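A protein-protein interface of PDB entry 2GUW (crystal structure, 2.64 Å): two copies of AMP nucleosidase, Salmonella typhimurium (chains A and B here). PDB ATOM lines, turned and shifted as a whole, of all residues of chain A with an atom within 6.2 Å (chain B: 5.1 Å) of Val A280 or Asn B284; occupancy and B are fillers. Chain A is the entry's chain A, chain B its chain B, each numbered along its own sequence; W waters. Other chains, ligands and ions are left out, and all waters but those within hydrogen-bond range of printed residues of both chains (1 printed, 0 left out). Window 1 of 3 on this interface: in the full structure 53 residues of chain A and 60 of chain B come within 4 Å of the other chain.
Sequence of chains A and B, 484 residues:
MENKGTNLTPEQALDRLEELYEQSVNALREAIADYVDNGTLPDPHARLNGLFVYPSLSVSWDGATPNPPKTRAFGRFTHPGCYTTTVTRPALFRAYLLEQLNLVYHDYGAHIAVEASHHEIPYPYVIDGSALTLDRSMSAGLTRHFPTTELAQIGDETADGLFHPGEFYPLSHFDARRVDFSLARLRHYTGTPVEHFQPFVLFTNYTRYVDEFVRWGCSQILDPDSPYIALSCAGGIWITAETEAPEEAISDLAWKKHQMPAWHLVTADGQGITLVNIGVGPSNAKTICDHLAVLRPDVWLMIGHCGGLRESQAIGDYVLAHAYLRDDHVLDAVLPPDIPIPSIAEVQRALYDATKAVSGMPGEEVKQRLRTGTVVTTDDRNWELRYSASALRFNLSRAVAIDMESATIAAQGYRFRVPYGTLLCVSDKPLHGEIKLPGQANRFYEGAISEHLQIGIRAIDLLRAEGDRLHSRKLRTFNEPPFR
Ile A278 touches none of the printed residues of chain B. Val A280 touches just these residues of chain B: Gln B259 (3.1 Å) and Asn B284 (3.7 Å). Of the printed residues of chain B, Asp A379 touches Ser B283. Of the printed residues of chain A, Gln B259 touches Val A280 and Arg A381. Asn B284 touches two residues of chain A. The nearest printed residue of chain B that does not touch Val A280 is Ser B283 (5.5 Å). The nearest residue of chain A that does not touch Asn B284 is Gly A281 (5.3 Å).
Val A280 touches Asn B284, but with the chains exchanged Asn A284 does not touch Val B280 (4.6 Å). Pro A282 touches Ser B283, but with the chains exchanged Ser A283 does not touch Pro B282 (4.6 Å). Positions printed for both chains: 279, 280, 281, 282, 283 and 284.
Printed residues of chain A that touch a printed residue of chain B: Val A280, Pro A282, Asp A379, Arg A381 and Met A404. Hydrophobic or aromatic side chains of chain A that line the printed part of chain B: Val A280, Pro A282 and Met A404. Of the 13 printed residues of chain B, 4 touch a printed residue of chain A. Among the printed residues, 8 pairs touch across the chains. Among the printed residues, no Asp or Glu carboxylate lies within 4 Å of a Lys or Arg side-chain nitrogen of the other chain.
The backbone NH of Arg A381 sits close to the side-chain sulfur of Met A404 (3.8 Å). OD1 of Asn B284 lies within hydrogen-bond range of NE2 of Gln B259 (2.5 Å). The side-chain hydroxyl (OG1) of Thr B287 sits at hydrogen-bond distance from the backbone carbonyl oxygen (O) of Ser B283 (2.9 Å). The backbone carbonyl oxygen (O) of Val A280 sits close to the side-chain amide oxygen (OD1) of Asn A284.
Water W1 lies within hydrogen-bond range of NH2 of Arg A381 (2.6 Å), OG1 of Thr B287 (2.9 Å) and OD1 of Asn B284 (3.1 Å).
Val A280 touches Gln B259. Asn B284 touches Val A280 (ND2 to O, 3.7 Å). OG of Ser B283 touches CD of Pro A282, at 3.96 Å. Asn B284 touches Arg A381 (OD1 to NH2, 3.7 Å). Arg A381 touches Thr B287. Ser B283 touches Met A404 (OG to CE, 3.7 Å).
NH2 of Arg A381 lies close to NE2 of Gln B259 (2.5 Å). The backbone carbonyl oxygen (O) of Asp A379 lies close to the side-chain hydroxyl (OG) of Ser B283 (2.4 Å).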
ATOM      1  N   ASN A 205      11.261 -30.266   7.272  1.00  0.00           N
ATOM      2  CA  ASN A 205      10.221 -30.587   8.248  1.00  0.00           C
ATOM      3  C   ASN A 205      10.746 -31.580   9.280  1.00  0.00           C
ATOM      4  O   ASN A 205       9.964 -32.209   9.988  1.00  0.00           O
ATOM      5  CB  ASN A 205       9.021 -31.197   7.511  1.00  0.00           C
ATOM      6  CG  ASN A 205       9.444 -32.258   6.495  1.00  0.00           C
ATOM      7  OD1 ASN A 205       8.629 -32.776   5.718  1.00  0.00           O
ATOM      8  ND2 ASN A 205      10.736 -32.588   6.498  1.00  0.00           N
ATOM      9  N   ILE A 278      10.263 -25.094   8.539  1.00  0.00           N
ATOM     10  CA  ILE A 278       8.908 -24.556   8.513  1.00  0.00           C
ATOM     11  C   ILE A 278       7.902 -25.311   9.345  1.00  0.00           C
ATOM     12  O   ILE A 278       6.806 -24.813   9.589  1.00  0.00           O
ATOM     13  CB  ILE A 278       8.359 -24.469   7.079  1.00  0.00           C
ATOM     14  CG1 ILE A 278       8.376 -25.846   6.420  1.00  0.00           C
ATOM     15  CG2 ILE A 278       9.172 -23.469   6.273  1.00  0.00           C
ATOM     16  CD1 ILE A 278       8.032 -25.813   4.953  1.00  0.00           C
ATOM     17  N   GLY A 279       8.273 -26.502   9.795  1.00  0.00           N
ATOM     18  CA  GLY A 279       7.347 -27.280  10.576  1.00  0.00           C
ATOM     19  C   GLY A 279       6.423 -28.045   9.640  1.00  0.00           C
ATOM     20  O   GLY A 279       6.674 -28.148   8.421  1.00  0.00           O
ATOM     21  N   VAL A 280       5.336 -28.569  10.193  1.00  0.00           N
ATOM     22  CA  VAL A 280       4.417 -29.346   9.391  1.00  0.00           C
ATOM     23  C   VAL A 280       3.074 -28.670   9.157  1.00  0.00           C
ATOM     24  O   VAL A 280       2.578 -27.933  10.018  1.00  0.00           O
ATOM     25  CB  VAL A 280       4.235 -30.780  10.018  1.00  0.00           C
ATOM     26  CG1 VAL A 280       4.667 -30.759  11.468  1.00  0.00           C
ATOM     27  CG2 VAL A 280       2.781 -31.276   9.870  1.00  0.00           C
ATOM     28  N   GLY A 281       2.510 -28.907   7.972  1.00  0.00           N
ATOM     29  CA  GLY A 281       1.219 -28.341   7.644  1.00  0.00           C
ATOM     30  C   GLY A 281       1.267 -27.304   6.544  1.00  0.00           C
ATOM     31  O   GLY A 281       2.226 -26.535   6.450  1.00  0.00           O
ATOM     32  N   PRO A 282       0.236 -27.248   5.692  1.00  0.00           N
ATOM     33  CA  PRO A 282       0.237 -26.266   4.613  1.00  0.00           C
ATOM     34  C   PRO A 282       0.056 -24.845   5.124  1.00  0.00           C
ATOM     35  O   PRO A 282       0.504 -23.880   4.512  1.00  0.00           O
ATOM     36  CB  PRO A 282      -0.921 -26.734   3.732  1.00  0.00           C
ATOM     37  CG  PRO A 282      -1.845 -27.329   4.707  1.00  0.00           C
ATOM     38  CD  PRO A 282      -0.937 -28.128   5.588  1.00  0.00           C
ATOM     39  N   SER A 283      -0.600 -24.733   6.265  1.00  0.00           N
ATOM     40  CA  SER A 283      -0.876 -23.437   6.837  1.00  0.00           C
ATOM     41  C   SER A 283       0.357 -22.581   7.093  1.00  0.00           C
ATOM     42  O   SER A 283       0.445 -21.462   6.584  1.00  0.00           O
ATOM     43  CB  SER A 283      -1.693 -23.597   8.121  1.00  0.00           C
ATOM     44  OG  SER A 283      -1.710 -22.397   8.859  1.00  0.00           O
ATOM     45  N   ASN A 284       1.321 -23.058   7.859  1.00  0.00           N
ATOM     46  CA  ASN A 284       2.442 -22.170   8.077  1.00  0.00           C
ATOM     47  C   ASN A 284       3.513 -22.275   7.006  1.00  0.00           C
ATOM     48  O   ASN A 284       4.535 -21.602   7.072  1.00  0.00           O
ATOM     49  CB  ASN A 284       2.995 -22.292   9.519  1.00  0.00           C
ATOM     50  CG  ASN A 284       3.269 -23.713   9.935  1.00  0.00           C
ATOM     51  OD1 ASN A 284       2.607 -24.656   9.478  1.00  0.00           O
ATOM     52  ND2 ASN A 284       4.238 -23.881  10.832  1.00  0.00           N
ATOM     53  N   ASP A 379      -3.828 -31.023   4.103  1.00  0.00           N
ATOM     54  CA  ASP A 379      -3.798 -30.355   5.401  1.00  0.00           C
ATOM     55  C   ASP A 379      -4.345 -31.289   6.484  1.00  0.00           C
ATOM     56  O   ASP A 379      -4.521 -30.876   7.623  1.00  0.00           O
ATOM     57  CB  ASP A 379      -4.605 -29.041   5.377  1.00  0.00           C
ATOM     58  CG  ASP A 379      -6.100 -29.248   5.129  1.00  0.00           C
ATOM     59  OD1 ASP A 379      -6.501 -30.378   4.777  1.00  0.00           O
ATOM     60  OD2 ASP A 379      -6.871 -28.269   5.279  1.00  0.00           O
ATOM     61  N   ARG A 381      -3.247 -34.602   8.204  1.00  0.00           N
ATOM     62  CA  ARG A 381      -2.280 -35.662   8.383  1.00  0.00           C
ATOM     63  C   ARG A 381      -2.863 -37.069   8.536  1.00  0.00           C
ATOM     64  O   ARG A 381      -2.281 -38.035   8.058  1.00  0.00           O
ATOM     65  CB  ARG A 381      -1.377 -35.391   9.574  1.00  0.00           C
ATOM     66  CG  ARG A 381      -0.351 -36.504   9.734  1.00  0.00           C
ATOM     67  CD  ARG A 381       0.986 -35.945  10.132  1.00  0.00           C
ATOM     68  NE  ARG A 381       0.814 -35.004  11.239  1.00  0.00           N
ATOM     69  CZ  ARG A 381       1.808 -34.406  11.886  1.00  0.00           C
ATOM     70  NH1 ARG A 381       3.072 -34.645  11.545  1.00  0.00           N
ATOM     71  NH2 ARG A 381       1.526 -33.562  12.871  1.00  0.00           N
ATOM     72  N   MET A 404       2.656 -32.913   3.443  1.00  0.00           N
ATOM     73  CA  MET A 404       1.879 -31.779   3.929  1.00  0.00           C
ATOM     74  C   MET A 404       2.389 -30.358   3.651  1.00  0.00           C
ATOM     75  O   MET A 404       1.873 -29.417   4.241  1.00  0.00           O
ATOM     76  CB  MET A 404       1.607 -31.953   5.431  1.00  0.00           C
ATOM     77  CG  MET A 404       0.678 -33.130   5.731  1.00  0.00           C
ATOM     78  SD  MET A 404       0.287 -33.428   7.480  1.00  0.00           S
ATOM     79  CE  MET A 404      -0.875 -32.027   7.893  1.00  0.00           C
ATOM     80  N   GLU A 405       3.374 -30.183   2.761  1.00  0.00           N
ATOM     81  CA  GLU A 405       3.858 -28.825   2.471  1.00  0.00           C
ATOM     82  C   GLU A 405       4.212 -28.505   1.022  1.00  0.00           C
ATOM     83  O   GLU A 405       4.121 -27.348   0.605  1.00  0.00           O
ATOM     84  CB  GLU A 405       5.064 -28.467   3.349  1.00  0.00           C
ATOM     85  CG  GLU A 405       4.828 -28.531   4.850  1.00  0.00           C
ATOM     86  CD  GLU A 405       5.002 -29.940   5.410  1.00  0.00           C
ATOM     87  OE1 GLU A 405       5.717 -30.753   4.778  1.00  0.00           O
ATOM     88  OE2 GLU A 405       4.438 -30.234   6.489  1.00  0.00           O
ATOM     89  N   GLN B 259       6.459 -32.284  18.476  1.00  0.00           N
ATOM     90  CA  GLN B 259       5.586 -31.365  17.764  1.00  0.00           C
ATOM     91  C   GLN B 259       4.536 -30.734  18.655  1.00  0.00           C
ATOM     92  O   GLN B 259       4.243 -29.549  18.511  1.00  0.00           O
ATOM     93  CB  GLN B 259       4.908 -32.109  16.623  1.00  0.00           C
ATOM     94  CG  GLN B 259       4.604 -31.272  15.410  1.00  0.00           C
ATOM     95  CD  GLN B 259       3.939 -32.086  14.307  1.00  0.00           C
ATOM     96  OE1 GLN B 259       4.425 -33.161  13.919  1.00  0.00           O
ATOM     97  NE2 GLN B 259       2.823 -31.576  13.794  1.00  0.00           N
ATOM     98  N   MET B 260       3.959 -31.510  19.567  1.00  0.00           N
ATOM     99  CA  MET B 260       2.942 -30.959  20.458  1.00  0.00           C
ATOM    100  C   MET B 260       3.151 -31.462  21.880  1.00  0.00           C
ATOM    101  O   MET B 260       2.333 -32.204  22.424  1.00  0.00           O
ATOM    102  CB  MET B 260       1.550 -31.336  19.955  1.00  0.00           C
ATOM    103  CG  MET B 260       1.167 -30.674  18.655  1.00  0.00           C
ATOM    104  SD  MET B 260      -0.263 -31.469  17.877  1.00  0.00           S
ATOM    105  CE  MET B 260       0.564 -32.531  16.686  1.00  0.00           C
ATOM    106  N   GLY B 279       0.538 -26.521  18.515  1.00  0.00           N
ATOM    107  CA  GLY B 279       1.157 -25.351  17.934  1.00  0.00           C
ATOM    108  C   GLY B 279       0.163 -24.337  17.418  1.00  0.00           C
ATOM    109  O   GLY B 279      -0.679 -23.806  18.155  1.00  0.00           O
ATOM    110  N   VAL B 280       0.256 -24.090  16.119  1.00  0.00           N
ATOM    111  CA  VAL B 280      -0.604 -23.126  15.469  1.00  0.00           C
ATOM    112  C   VAL B 280      -1.248 -23.779  14.254  1.00  0.00           C
ATOM    113  O   VAL B 280      -0.656 -24.671  13.647  1.00  0.00           O
ATOM    114  CB  VAL B 280       0.241 -21.943  15.003  1.00  0.00           C
ATOM    115  CG1 VAL B 280       1.344 -22.471  14.081  1.00  0.00           C
ATOM    116  CG2 VAL B 280      -0.631 -20.894  14.301  1.00  0.00           C
ATOM    117  N   GLY B 281      -2.457 -23.346  13.907  1.00  0.00           N
ATOM    118  CA  GLY B 281      -3.108 -23.894  12.731  1.00  0.00           C
ATOM    119  C   GLY B 281      -4.139 -24.979  12.963  1.00  0.00           C
ATOM    120  O   GLY B 281      -4.080 -25.696  13.950  1.00  0.00           O
ATOM    121  N   PRO B 282      -5.103 -25.115  12.042  1.00  0.00           N
ATOM    122  CA  PRO B 282      -6.178 -26.107  12.105  1.00  0.00           C
ATOM    123  C   PRO B 282      -5.692 -27.544  11.926  1.00  0.00           C
ATOM    124  O   PRO B 282      -6.271 -28.471  12.469  1.00  0.00           O
ATOM    125  CB  PRO B 282      -7.104 -25.676  10.972  1.00  0.00           C
ATOM    126  CG  PRO B 282      -6.844 -24.227  10.840  1.00  0.00           C
ATOM    127  CD  PRO B 282      -5.359 -24.152  10.961  1.00  0.00           C
ATOM    128  N   SER B 283      -4.635 -27.727  11.150  1.00  0.00           N
ATOM    129  CA  SER B 283      -4.111 -29.067  10.896  1.00  0.00           C
ATOM    130  C   SER B 283      -3.775 -29.836  12.163  1.00  0.00           C
ATOM    131  O   SER B 283      -4.297 -30.928  12.424  1.00  0.00           O
ATOM    132  CB  SER B 283      -2.846 -28.997  10.038  1.00  0.00           C
ATOM    133  OG  SER B 283      -3.139 -29.241   8.681  1.00  0.00           O
ATOM    134  N   ASN B 284      -2.889 -29.243  12.946  1.00  0.00           N
ATOM    135  CA  ASN B 284      -2.434 -29.858  14.159  1.00  0.00           C
ATOM    136  C   ASN B 284      -3.536 -30.081  15.166  1.00  0.00           C
ATOM    137  O   ASN B 284      -3.566 -31.107  15.837  1.00  0.00           O
ATOM    138  CB  ASN B 284      -1.273 -29.031  14.705  1.00  0.00           C
ATOM    139  CG  ASN B 284       0.013 -29.302  13.937  1.00  0.00           C
ATOM    140  OD1 ASN B 284       0.773 -30.198  14.302  1.00  0.00           O
ATOM    141  ND2 ASN B 284       0.239 -28.560  12.839  1.00  0.00           N
ATOM    142  N   ALA B 285      -4.458 -29.132  15.241  1.00  0.00           N
ATOM    143  CA  ALA B 285      -5.587 -29.237  16.156  1.00  0.00           C
ATOM    144  C   ALA B 285      -6.368 -30.511  15.802  1.00  0.00           C
ATOM    145  O   ALA B 285      -6.613 -31.374  16.662  1.00  0.00           O
ATOM    146  CB  ALA B 285      -6.479 -28.000  16.028  1.00  0.00           C
ATOM    147  N   LYS B 286      -6.732 -30.625  14.524  1.00  0.00           N
ATOM    148  CA  LYS B 286      -7.470 -31.774  14.024  1.00  0.00           C
ATOM    149  C   LYS B 286      -6.718 -33.058  14.369  1.00  0.00           C
ATOM    150  O   LYS B 286      -7.302 -34.022  14.861  1.00  0.00           O
ATOM    151  CB  LYS B 286      -7.627 -31.653  12.512  1.00  0.00           C
ATOM    152  CG  LYS B 286      -8.685 -32.548  11.878  1.00  0.00           C
ATOM    153  CD  LYS B 286      -8.185 -33.942  11.636  1.00  0.00           C
ATOM    154  CE  LYS B 286      -9.025 -34.624  10.570  1.00  0.00           C
ATOM    155  NZ  LYS B 286      -8.453 -35.944  10.169  1.00  0.00           N
ATOM    156  N   THR B 287      -5.414 -33.040  14.123  1.00  0.00           N
ATOM    157  CA  THR B 287      -4.528 -34.178  14.374  1.00  0.00           C
ATOM    158  C   THR B 287      -4.490 -34.683  15.810  1.00  0.00           C
ATOM    159  O   THR B 287      -4.748 -35.866  16.070  1.00  0.00           O
ATOM    160  CB  THR B 287      -3.077 -33.846  14.014  1.00  0.00           C
ATOM    161  OG1 THR B 287      -2.992 -33.532  12.626  1.00  0.00           O
ATOM    162  CG2 THR B 287      -2.159 -35.020  14.340  1.00  0.00           C
ATOM    163  N   ILE B 288      -4.138 -33.791  16.734  1.00  0.00           N
ATOM    164  CA  ILE B 288      -4.036 -34.197  18.115  1.00  0.00           C
ATOM    165  C   ILE B 288      -5.382 -34.721  18.606  1.00  0.00           C
ATOM    166  O   ILE B 288      -5.427 -35.720  19.327  1.00  0.00           O
ATOM    167  CB  ILE B 288      -3.502 -33.033  19.034  1.00  0.00           C
ATOM    168  CG1 ILE B 288      -3.217 -33.579  20.439  1.00  0.00           C
ATOM    169  CG2 ILE B 288      -4.499 -31.886  19.117  1.00  0.00           C
ATOM    170  CD1 ILE B 288      -1.997 -34.440  20.496  1.00  0.00           C
ATOM    171  N   CYS B 289      -6.475 -34.077  18.190  1.00  0.00           N
ATOM    172  CA  CYS B 289      -7.801 -34.510  18.619  1.00  0.00           C
ATOM    173  C   CYS B 289      -8.194 -35.883  18.142  1.00  0.00           C
ATOM    174  O   CYS B 289      -8.876 -36.595  18.866  1.00  0.00           O
ATOM    175  CB  CYS B 289      -8.861 -33.513  18.199  1.00  0.00           C
ATOM    176  SG  CYS B 289      -8.850 -32.112  19.304  1.00  0.00           S
HETATM  177  O   HOH W   1      -0.520 -32.141  12.220  1.00  0.00           O
